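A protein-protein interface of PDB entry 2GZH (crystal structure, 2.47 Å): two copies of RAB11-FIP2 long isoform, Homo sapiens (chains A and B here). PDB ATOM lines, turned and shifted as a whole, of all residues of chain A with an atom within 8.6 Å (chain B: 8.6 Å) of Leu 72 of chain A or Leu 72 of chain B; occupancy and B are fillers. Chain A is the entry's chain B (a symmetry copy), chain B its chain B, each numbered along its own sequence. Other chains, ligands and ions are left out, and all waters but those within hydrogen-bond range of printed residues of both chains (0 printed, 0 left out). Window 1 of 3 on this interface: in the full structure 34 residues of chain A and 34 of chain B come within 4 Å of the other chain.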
ATOM      1  N   LYS A  65       9.860  26.165 -19.777  1.00  0.00           N
ATOM      2  CA  LYS A  65      11.017  26.422 -18.970  1.00  0.00           C
ATOM      3  C   LYS A  65      10.890  27.810 -18.389  1.00  0.00           C
ATOM      4  O   LYS A  65      11.096  27.984 -17.200  1.00  0.00           O
ATOM      5  CB  LYS A  65      12.309  26.321 -19.783  1.00  0.00           C
ATOM      6  CG  LYS A  65      12.631  24.959 -20.353  1.00  0.00           C
ATOM      7  CD  LYS A  65      12.883  23.965 -19.255  1.00  0.00           C
ATOM      8  CE  LYS A  65      12.944  22.510 -19.734  1.00  0.00           C
ATOM      9  NZ  LYS A  65      12.651  21.678 -18.542  1.00  0.00           N
ATOM     10  N   ASP A  66      10.544  28.791 -19.229  1.00  0.00           N
ATOM     11  CA  ASP A  66      10.243  30.170 -18.790  1.00  0.00           C
ATOM     12  C   ASP A  66       9.241  30.231 -17.648  1.00  0.00           C
ATOM     13  O   ASP A  66       9.496  30.886 -16.606  1.00  0.00           O
ATOM     14  CB  ASP A  66       9.750  31.005 -19.948  1.00  0.00           C
ATOM     15  CG  ASP A  66      10.872  31.356 -20.935  1.00  0.00           C
ATOM     16  OD1 ASP A  66      12.081  31.405 -20.565  1.00  0.00           O
ATOM     17  OD2 ASP A  66      10.531  31.581 -22.112  1.00  0.00           O
ATOM     18  N   THR A  67       8.135  29.523 -17.821  1.00  0.00           N
ATOM     19  CA  THR A  67       7.095  29.487 -16.813  1.00  0.00           C
ATOM     20  C   THR A  67       7.684  28.980 -15.506  1.00  0.00           C
ATOM     21  O   THR A  67       7.522  29.623 -14.444  1.00  0.00           O
ATOM     22  CB  THR A  67       5.966  28.638 -17.306  1.00  0.00           C
ATOM     23  OG1 THR A  67       5.452  29.251 -18.488  1.00  0.00           O
ATOM     24  CG2 THR A  67       4.847  28.527 -16.290  1.00  0.00           C
ATOM     25  N   HIS A  68       8.452  27.885 -15.603  1.00  0.00           N
ATOM     26  CA  HIS A  68       9.088  27.312 -14.445  1.00  0.00           C
ATOM     27  C   HIS A  68      10.073  28.264 -13.777  1.00  0.00           C
ATOM     28  O   HIS A  68      10.115  28.319 -12.540  1.00  0.00           O
ATOM     29  CB  HIS A  68       9.771  25.992 -14.765  1.00  0.00           C
ATOM     30  CG  HIS A  68      10.115  25.203 -13.533  1.00  0.00           C
ATOM     31  ND1 HIS A  68      11.300  24.509 -13.393  1.00  0.00           N
ATOM     32  CD2 HIS A  68       9.427  25.013 -12.377  1.00  0.00           C
ATOM     33  CE1 HIS A  68      11.334  23.933 -12.204  1.00  0.00           C
ATOM     34  NE2 HIS A  68      10.199  24.203 -11.573  1.00  0.00           N
ATOM     35  N   ILE A  69      10.859  28.987 -14.587  1.00  0.00           N
ATOM     36  CA  ILE A  69      11.759  30.010 -14.070  1.00  0.00           C
ATOM     37  C   ILE A  69      10.985  31.085 -13.271  1.00  0.00           C
ATOM     38  O   ILE A  69      11.361  31.427 -12.142  1.00  0.00           O
ATOM     39  CB  ILE A  69      12.584  30.618 -15.182  1.00  0.00           C
ATOM     40  CG1 ILE A  69      13.506  29.532 -15.798  1.00  0.00           C
ATOM     41  CG2 ILE A  69      13.300  31.910 -14.697  1.00  0.00           C
ATOM     42  CD1 ILE A  69      14.306  29.983 -17.083  1.00  0.00           C
ATOM     43  N   ARG A  70       9.883  31.562 -13.828  1.00  0.00           N
ATOM     44  CA  ARG A  70       8.999  32.477 -13.124  1.00  0.00           C
ATOM     45  C   ARG A  70       8.430  31.939 -11.814  1.00  0.00           C
ATOM     46  O   ARG A  70       8.428  32.660 -10.804  1.00  0.00           O
ATOM     47  CB  ARG A  70       7.859  32.983 -14.023  1.00  0.00           C
ATOM     48  CG  ARG A  70       8.347  34.049 -14.991  1.00  0.00           C
ATOM     49  CD  ARG A  70       7.214  34.675 -15.797  1.00  0.00           C
ATOM     50  NE  ARG A  70       6.913  33.771 -16.920  1.00  0.00           N
ATOM     51  CZ  ARG A  70       5.750  33.180 -17.045  1.00  0.00           C
ATOM     52  NH1 ARG A  70       4.847  33.445 -16.140  1.00  0.00           N
ATOM     53  NH2 ARG A  70       5.486  32.368 -18.031  1.00  0.00           N
ATOM     54  N   GLU A  71       7.932  30.718 -11.832  1.00  0.00           N
ATOM     55  CA  GLU A  71       7.504  30.064 -10.606  1.00  0.00           C
ATOM     56  C   GLU A  71       8.624  29.997  -9.561  1.00  0.00           C
ATOM     57  O   GLU A  71       8.407  30.344  -8.395  1.00  0.00           O
ATOM     58  CB  GLU A  71       6.980  28.659 -10.904  1.00  0.00           C
ATOM     59  CG  GLU A  71       5.659  28.628 -11.742  1.00  0.00           C
ATOM     60  CD  GLU A  71       5.362  27.208 -12.315  1.00  0.00           C
ATOM     61  OE1 GLU A  71       6.292  26.343 -12.459  1.00  0.00           O
ATOM     62  OE2 GLU A  71       4.177  26.959 -12.637  1.00  0.00           O
ATOM     63  N   LEU A  72       9.817  29.576  -9.967  1.00  0.00           N
ATOM     64  CA  LEU A  72      10.979  29.576  -9.073  1.00  0.00           C
ATOM     65  C   LEU A  72      11.298  30.960  -8.512  1.00  0.00           C
ATOM     66  O   LEU A  72      11.569  31.116  -7.305  1.00  0.00           O
ATOM     67  CB  LEU A  72      12.226  28.989  -9.759  1.00  0.00           C
ATOM     68  CG  LEU A  72      12.136  27.463 -10.049  1.00  0.00           C
ATOM     69  CD1 LEU A  72      13.286  26.989 -10.951  1.00  0.00           C
ATOM     70  CD2 LEU A  72      12.102  26.672  -8.786  1.00  0.00           C
ATOM     71  N   GLU A  73      11.250  31.964  -9.391  1.00  0.00           N
ATOM     72  CA  GLU A  73      11.513  33.343  -8.979  1.00  0.00           C
ATOM     73  C   GLU A  73      10.489  33.817  -7.976  1.00  0.00           C
ATOM     74  O   GLU A  73      10.847  34.414  -6.979  1.00  0.00           O
ATOM     75  CB  GLU A  73      11.545  34.246 -10.194  1.00  0.00           C
ATOM     76  CG  GLU A  73      12.861  34.129 -10.946  1.00  0.00           C
ATOM     77  CD  GLU A  73      12.821  34.822 -12.293  1.00  0.00           C
ATOM     78  OE1 GLU A  73      11.725  35.271 -12.738  1.00  0.00           O
ATOM     79  OE2 GLU A  73      13.896  34.892 -12.927  1.00  0.00           O
ATOM     80  N   ASP A  74       9.218  33.508  -8.200  1.00  0.00           N
ATOM     81  CA  ASP A  74       8.201  33.999  -7.307  1.00  0.00           C
ATOM     82  C   ASP A  74       8.369  33.352  -5.939  1.00  0.00           C
ATOM     83  O   ASP A  74       8.133  33.996  -4.928  1.00  0.00           O
ATOM     84  CB  ASP A  74       6.800  33.702  -7.843  1.00  0.00           C
ATOM     85  CG  ASP A  74       6.476  34.487  -9.103  1.00  0.00           C
ATOM     86  OD1 ASP A  74       7.230  35.434  -9.460  1.00  0.00           O
ATOM     87  OD2 ASP A  74       5.457  34.142  -9.761  1.00  0.00           O
ATOM     88  N   TYR A  75       8.718  32.064  -5.927  1.00  0.00           N
ATOM     89  CA  TYR A  75       8.811  31.337  -4.691  1.00  0.00           C
ATOM     90  C   TYR A  75       9.953  31.943  -3.873  1.00  0.00           C
ATOM     91  O   TYR A  75       9.839  32.173  -2.680  1.00  0.00           O
ATOM     92  CB  TYR A  75       9.071  29.849  -4.975  1.00  0.00           C
ATOM     93  CG  TYR A  75       9.366  29.104  -3.734  1.00  0.00           C
ATOM     94  CD1 TYR A  75       8.341  28.522  -2.985  1.00  0.00           C
ATOM     95  CD2 TYR A  75      10.675  29.027  -3.250  1.00  0.00           C
ATOM     96  CE1 TYR A  75       8.623  27.825  -1.777  1.00  0.00           C
ATOM     97  CE2 TYR A  75      10.974  28.339  -2.079  1.00  0.00           C
ATOM     98  CZ  TYR A  75       9.946  27.744  -1.330  1.00  0.00           C
ATOM     99  OH  TYR A  75      10.262  27.093  -0.125  1.00  0.00           O
ATOM    100  N   ILE A  76      11.080  32.148  -4.519  1.00  0.00           N
ATOM    101  CA  ILE A  76      12.189  32.852  -3.913  1.00  0.00           C
ATOM    102  C   ILE A  76      11.753  34.207  -3.315  1.00  0.00           C
ATOM    103  O   ILE A  76      12.009  34.481  -2.133  1.00  0.00           O
ATOM    104  CB  ILE A  76      13.329  33.027  -4.950  1.00  0.00           C
ATOM    105  CG1 ILE A  76      13.958  31.646  -5.197  1.00  0.00           C
ATOM    106  CG2 ILE A  76      14.378  34.025  -4.442  1.00  0.00           C
ATOM    107  CD1 ILE A  76      15.054  31.547  -6.316  1.00  0.00           C
ATOM    108  N   ASP A  77      11.097  35.051  -4.097  1.00  0.00           N
ATOM    109  CA  ASP A  77      10.739  36.353  -3.592  1.00  0.00           C
ATOM    110  C   ASP A  77       9.800  36.269  -2.407  1.00  0.00           C
ATOM    111  O   ASP A  77       9.966  36.995  -1.429  1.00  0.00           O
ATOM    112  CB  ASP A  77      10.088  37.197  -4.701  1.00  0.00           C
ATOM    113  CG  ASP A  77      11.126  37.835  -5.642  1.00  0.00           C
ATOM    114  OD1 ASP A  77      12.372  37.681  -5.391  1.00  0.00           O
ATOM    115  OD2 ASP A  77      10.685  38.480  -6.649  1.00  0.00           O
ATOM    116  N   ASN A  78       8.809  35.397  -2.489  1.00  0.00           N
ATOM    117  CA  ASN A  78       7.887  35.252  -1.386  1.00  0.00           C
ATOM    118  C   ASN A  78       8.519  34.665  -0.156  1.00  0.00           C
ATOM    119  O   ASN A  78       8.131  35.020   0.934  1.00  0.00           O
ATOM    120  CB  ASN A  78       6.670  34.427  -1.743  1.00  0.00           C
ATOM    121  CG  ASN A  78       5.844  35.058  -2.858  1.00  0.00           C
ATOM    122  OD1 ASN A  78       5.392  34.350  -3.741  1.00  0.00           O
ATOM    123  ND2 ASN A  78       5.669  36.386  -2.841  1.00  0.00           N
ATOM    124  N   LEU A  79       9.500  33.787  -0.323  1.00  0.00           N
ATOM    125  CA  LEU A  79      10.185  33.272   0.821  1.00  0.00           C
ATOM    126  C   LEU A  79      11.113  34.375   1.419  1.00  0.00           C
ATOM    127  O   LEU A  79      11.212  34.515   2.643  1.00  0.00           O
ATOM    128  CB  LEU A  79      10.968  32.031   0.424  1.00  0.00           C
ATOM    129  CG  LEU A  79      11.932  31.440   1.456  1.00  0.00           C
ATOM    130  CD1 LEU A  79      11.175  30.854   2.691  1.00  0.00           C
ATOM    131  CD2 LEU A  79      12.849  30.373   0.787  1.00  0.00           C
ATOM    132  N   LYS B  65      18.542  27.948 -20.186  1.00  0.00           N
ATOM    133  CA  LYS B  65      17.398  28.011 -19.324  1.00  0.00           C
ATOM    134  C   LYS B  65      17.537  26.938 -18.272  1.00  0.00           C
ATOM    135  O   LYS B  65      17.349  27.218 -17.101  1.00  0.00           O
ATOM    136  CB  LYS B  65      16.094  27.807 -20.098  1.00  0.00           C
ATOM    137  CG  LYS B  65      15.759  28.862 -21.128  1.00  0.00           C
ATOM    138  CD  LYS B  65      15.521  30.193 -20.473  1.00  0.00           C
ATOM    139  CE  LYS B  65      15.449  31.367 -21.457  1.00  0.00           C
ATOM    140  NZ  LYS B  65      15.757  32.581 -20.663  1.00  0.00           N
ATOM    141  N   ASP B  66      17.874  25.714 -18.693  1.00  0.00           N
ATOM    142  CA  ASP B  66      18.185  24.596 -17.778  1.00  0.00           C
ATOM    143  C   ASP B  66      19.203  24.960 -16.710  1.00  0.00           C
ATOM    144  O   ASP B  66      18.966  24.740 -15.496  1.00  0.00           O
ATOM    145  CB  ASP B  66      18.663  23.390 -18.550  1.00  0.00           C
ATOM    146  CG  ASP B  66      17.528  22.701 -19.321  1.00  0.00           C
ATOM    147  OD1 ASP B  66      16.325  22.796 -18.941  1.00  0.00           O
ATOM    148  OD2 ASP B  66      17.852  22.053 -20.335  1.00  0.00           O
ATOM    149  N   THR B  67      20.305  25.551 -17.150  1.00  0.00           N
ATOM    150  CA  THR B  67      21.360  25.955 -16.243  1.00  0.00           C
ATOM    151  C   THR B  67      20.788  26.912 -15.209  1.00  0.00           C
ATOM    152  O   THR B  67      20.968  26.709 -13.985  1.00  0.00           O
ATOM    153  CB  THR B  67      22.479  26.557 -17.032  1.00  0.00           C
ATOM    154  OG1 THR B  67      22.977  25.548 -17.909  1.00  0.00           O
ATOM    155  CG2 THR B  67      23.612  27.034 -16.146  1.00  0.00           C
ATOM    156  N   HIS B  68      20.016  27.896 -15.693  1.00  0.00           N
ATOM    157  CA  HIS B  68      19.395  28.859 -14.821  1.00  0.00           C
ATOM    158  C   HIS B  68      18.424  28.226 -13.833  1.00  0.00           C
ATOM    159  O   HIS B  68      18.400  28.633 -12.664  1.00  0.00           O
ATOM    160  CB  HIS B  68      18.704  29.968 -15.598  1.00  0.00           C
ATOM    161  CG  HIS B  68      18.376  31.158 -14.742  1.00  0.00           C
ATOM    162  ND1 HIS B  68      17.192  31.858 -14.852  1.00  0.00           N
ATOM    163  CD2 HIS B  68      19.081  31.762 -13.749  1.00  0.00           C
ATOM    164  CE1 HIS B  68      17.173  32.835 -13.961  1.00  0.00           C
ATOM    165  NE2 HIS B  68      18.318  32.815 -13.292  1.00  0.00           N
ATOM    166  N   ILE B  69      17.627  27.255 -14.305  1.00  0.00           N
ATOM    167  CA  ILE B  69      16.739  26.500 -13.432  1.00  0.00           C
ATOM    168  C   ILE B  69      17.527  25.796 -12.304  1.00  0.00           C
ATOM    169  O   ILE B  69      17.169  25.899 -11.122  1.00  0.00           O
ATOM    170  CB  ILE B  69      15.899  25.526 -14.227  1.00  0.00           C
ATOM    171  CG1 ILE B  69      14.964  26.307 -15.188  1.00  0.00           C
ATOM    172  CG2 ILE B  69      15.194  24.507 -13.288  1.00  0.00           C
ATOM    173  CD1 ILE B  69      14.147  25.414 -16.203  1.00  0.00           C
ATOM    174  N   ARG B  70      18.622  25.143 -12.660  1.00  0.00           N
ATOM    175  CA  ARG B  70      19.519  24.552 -11.680  1.00  0.00           C
ATOM    176  C   ARG B  70      20.106  25.537 -10.672  1.00  0.00           C
ATOM    177  O   ARG B  70      20.125  25.241  -9.466  1.00  0.00           O
ATOM    178  CB  ARG B  70      20.647  23.745 -12.344  1.00  0.00           C
ATOM    179  CG  ARG B  70      20.148  22.398 -12.839  1.00  0.00           C
ATOM    180  CD  ARG B  70      21.271  21.514 -13.372  1.00  0.00           C
ATOM    181  NE  ARG B  70      21.553  21.936 -14.755  1.00  0.00           N
ATOM    182  CZ  ARG B  70      22.712  22.435 -15.107  1.00  0.00           C
ATOM    183  NH1 ARG B  70      23.629  22.522 -14.182  1.00  0.00           N
ATOM    184  NH2 ARG B  70      22.959  22.823 -16.327  1.00  0.00           N
ATOM    185  N   GLU B  71      20.599  26.662 -11.149  1.00  0.00           N
ATOM    186  CA  GLU B  71      21.044  27.723 -10.259  1.00  0.00           C
ATOM    187  C   GLU B  71      19.939  28.176  -9.297  1.00  0.00           C
ATOM    188  O   GLU B  71      20.174  28.286  -8.089  1.00  0.00           O
ATOM    189  CB  GLU B  71      21.560  28.916 -11.065  1.00  0.00           C
ATOM    190  CG  GLU B  71      22.868  28.630 -11.873  1.00  0.00           C
ATOM    191  CD  GLU B  71      23.153  29.735 -12.937  1.00  0.00           C
ATOM    192  OE1 GLU B  71      22.218  30.487 -13.378  1.00  0.00           O
ATOM    193  OE2 GLU B  71      24.332  29.843 -13.345  1.00  0.00           O
ATOM    194  N   LEU B  72      18.739  28.420  -9.813  1.00  0.00           N
ATOM    195  CA  LEU B  72      17.590  28.755  -8.965  1.00  0.00           C
ATOM    196  C   LEU B  72      17.284  27.679  -7.927  1.00  0.00           C
ATOM    197  O   LEU B  72      17.031  27.983  -6.744  1.00  0.00           O
ATOM    198  CB  LEU B  72      16.332  29.049  -9.801  1.00  0.00           C
ATOM    199  CG  LEU B  72      16.413  30.359 -10.639  1.00  0.00           C
ATOM    200  CD1 LEU B  72      15.248  30.467 -11.635  1.00  0.00           C
ATOM    201  CD2 LEU B  72      16.463  31.561  -9.760  1.00  0.00           C
ATOM    202  N   GLU B  73      17.322  26.420  -8.370  1.00  0.00           N
ATOM    203  CA  GLU B  73      17.069  25.294  -7.472  1.00  0.00           C
ATOM    204  C   GLU B  73      18.109  25.222  -6.380  1.00  0.00           C
ATOM    205  O   GLU B  73      17.767  25.038  -5.228  1.00  0.00           O
ATOM    206  CB  GLU B  73      17.021  24.004  -8.266  1.00  0.00           C
ATOM    207  CG  GLU B  73      15.694  23.838  -8.987  1.00  0.00           C
ATOM    208  CD  GLU B  73      15.717  22.694  -9.981  1.00  0.00           C
ATOM    209  OE1 GLU B  73      16.806  22.108 -10.245  1.00  0.00           O
ATOM    210  OE2 GLU B  73      14.633  22.396 -10.529  1.00  0.00           O
ATOM    211  N   ASP B  74      19.375  25.422  -6.721  1.00  0.00           N
ATOM    212  CA  ASP B  74      20.406  25.295  -5.725  1.00  0.00           C
ATOM    213  C   ASP B  74      20.257  26.404  -4.693  1.00  0.00           C
ATOM    214  O   ASP B  74      20.510  26.181  -3.518  1.00  0.00           O
ATOM    215  CB  ASP B  74      21.799  25.368  -6.354  1.00  0.00           C
ATOM    216  CG  ASP B  74      22.106  24.171  -7.238  1.00  0.00           C
ATOM    217  OD1 ASP B  74      21.350  23.161  -7.207  1.00  0.00           O
ATOM    218  OD2 ASP B  74      23.114  24.244  -7.992  1.00  0.00           O
ATOM    219  N   TYR B  75      19.904  27.605  -5.155  1.00  0.00           N
ATOM    220  CA  TYR B  75      19.828  28.739  -4.275  1.00  0.00           C
ATOM    221  C   TYR B  75      18.700  28.483  -3.274  1.00  0.00           C
ATOM    222  O   TYR B  75      18.832  28.712  -2.083  1.00  0.00           O
ATOM    223  CB  TYR B  75      19.559  30.017  -5.087  1.00  0.00           C
ATOM    224  CG  TYR B  75      19.280  31.170  -4.207  1.00  0.00           C
ATOM    225  CD1 TYR B  75      20.315  31.986  -3.743  1.00  0.00           C
ATOM    226  CD2 TYR B  75      17.978  31.425  -3.767  1.00  0.00           C
ATOM    227  CE1 TYR B  75      20.048  33.081  -2.875  1.00  0.00           C
ATOM    228  CE2 TYR B  75      17.694  32.498  -2.930  1.00  0.00           C
ATOM    229  CZ  TYR B  75      18.732  33.326  -2.471  1.00  0.00           C
ATOM    230  OH  TYR B  75      18.432  34.378  -1.589  1.00  0.00           O
ATOM    231  N   ILE B  76      17.564  28.056  -3.781  1.00  0.00           N
ATOM    232  CA  ILE B  76      16.465  27.631  -2.941  1.00  0.00           C
ATOM    233  C   ILE B  76      16.914  26.593  -1.890  1.00  0.00           C
ATOM    234  O   ILE B  76      16.677  26.778  -0.686  1.00  0.00           O
ATOM    235  CB  ILE B  76      15.311  27.087  -3.822  1.00  0.00           C
ATOM    236  CG1 ILE B  76      14.675  28.279  -4.555  1.00  0.00           C
ATOM    237  CG2 ILE B  76      14.273  26.351  -2.965  1.00  0.00           C
ATOM    238  CD1 ILE B  76      13.562  27.959  -5.614  1.00  0.00           C
ATOM    239  N   ASP B  77      17.561  25.517  -2.312  1.00  0.00           N
ATOM    240  CA  ASP B  77      17.931  24.495  -1.366  1.00  0.00           C
ATOM    241  C   ASP B  77      18.887  25.010  -0.310  1.00  0.00           C
ATOM    242  O   ASP B  77      18.737  24.699   0.870  1.00  0.00           O
ATOM    243  CB  ASP B  77      18.567  23.297  -2.091  1.00  0.00           C
ATOM    244  CG  ASP B  77      17.517  22.358  -2.713  1.00  0.00           C
ATOM    245  OD1 ASP B  77      16.275  22.599  -2.519  1.00  0.00           O
ATOM    246  OD2 ASP B  77      17.945  21.385  -3.415  1.00  0.00           O
ATOM    247  N   ASN B  78      19.874  25.786  -0.725  1.00  0.00           N
ATOM    248  CA  ASN B  78      20.811  26.327   0.232  1.00  0.00           C
ATOM    249  C   ASN B  78      20.196  27.331   1.166  1.00  0.00           C
ATOM    250  O   ASN B  78      20.601  27.404   2.304  1.00  0.00           O
ATOM    251  CB  ASN B  78      22.020  26.957  -0.423  1.00  0.00           C
ATOM    252  CG  ASN B  78      22.832  25.956  -1.236  1.00  0.00           C
ATOM    253  OD1 ASN B  78      23.269  26.284  -2.325  1.00  0.00           O
ATOM    254  ND2 ASN B  78      23.010  24.729  -0.731  1.00  0.00           N
ATOM    255  N   LEU B  79      19.210  28.086   0.699  1.00  0.00           N
ATOM    256  CA  LEU B  79      18.540  28.991   1.581  1.00  0.00           C
ATOM    257  C   LEU B  79      17.625  28.192   2.559  1.00  0.00           C
ATOM    258  O   LEU B  79      17.544  28.516   3.749  1.00  0.00           O
ATOM    259  CB  LEU B  79      17.748  29.999   0.763  1.00  0.00           C
ATOM    260  CG  LEU B  79      16.798  30.933   1.516  1.00  0.00           C
ATOM    261  CD1 LEU B  79      17.572  31.933   2.434  1.00  0.00           C
ATOM    262  CD2 LEU B  79      15.868  31.678   0.512  1.00  0.00           C
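Among the printed residues, pairs that only touch across the chains: Lys 65 of chain A with Ile 69 of chain B (3.6 Å), His 68 of chain A with Ile 69 of chain B (3.9 Å), Ile 69 of chain A with Lys 65 of chain B (3.6 Å), Ile 69 of chain A with His 68 of chain B (3.9 Å), Ile 69 of chain A with Ile 69 of chain B (3.6 Å), Ile 69 of chain A with Leu 72 of chain B (3.9 Å), Leu 72 of chain A with Ile 69 of chain B (3.9 Å), Leu 72 of chain A with Leu 72 of chain B (3.9 Å), Leu 72 of chain A with Ile 76 of chain B (3.7 Å), Tyr 75 of chain A with Ile 76 of chain B (3.9 Å), Ile 76 of chain A with Leu 72 of chain B (3.7 Å), Ile 76 of chain A with Tyr 75 of chain B (3.9 Å), Ile 76 of chain A with Ile 76 of chain B (3.5 Å) and Leu 79 of chain A with Leu 79 of chain B (3.3 Å).
Of the 15 printed residues of chain B, 8 touch a printed residue of chain A. Of the 15 printed residues of chain A, 8 touch a printed residue of chain B. Printed residues of chain A that touch a printed residue of chain B: Lys 65, Asp 66, His 68, Ile 69, Leu 72, Tyr 75, Ile 76 and Leu 79. Among the printed residues, 16 pairs touch across the chains.
Lys 65 of chain A touches Asp 66 of chain B, and with the chains exchanged Asp 66 of chain A touches Lys 65 of chain B. Leu 72 of chain A touches Ile 76 of chain B, and with the chains exchanged Ile 76 of chain A touches Leu 72 of chain B. Tyr 75 of chain A touches Ile 76 of chain B, and with the chains exchanged Ile 76 of chain A touches Tyr 75 of chain B. Leu 79 of chain A touches its own counterpart, Leu 79 of chain B.
Of the printed residues of chain B, His 68 of chain A touches Ile 69 (3.9 Å). Printed residues of chain B within 4 Å of Ile 69 of chain A: Lys 65, His 68, Ile 69 and Leu 72. Leu 72 of chain A touches three residues of chain B. Of the printed residues of chain B, Leu 79 of chain A touches Leu 79. Printed residues of chain A within 4 Å of His 68 of chain B: Ile 69. Leu 72 of chain B touches just these residues of chain A: Ile 69 (3.9 Å), Leu 72 (3.9 Å) and Ile 76 (3.7 Å). Asn 78 of chain B touches none of the printed residues of chain A. The nearest residue of chain A that does not touch Leu 72 of chain B is Glu 73 of chain A (4.4 Å).
The side-chain carboxylate (OD1) of Asp 66 of chain A lies within salt-bridge range of the side-chain amino group (NZ) of Lys 65 of chain B (3.9 Å). OD1 of Asp 66 of chain B lies within salt-bridge range of NZ of Lys 65 of chain A (3.9 Å).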
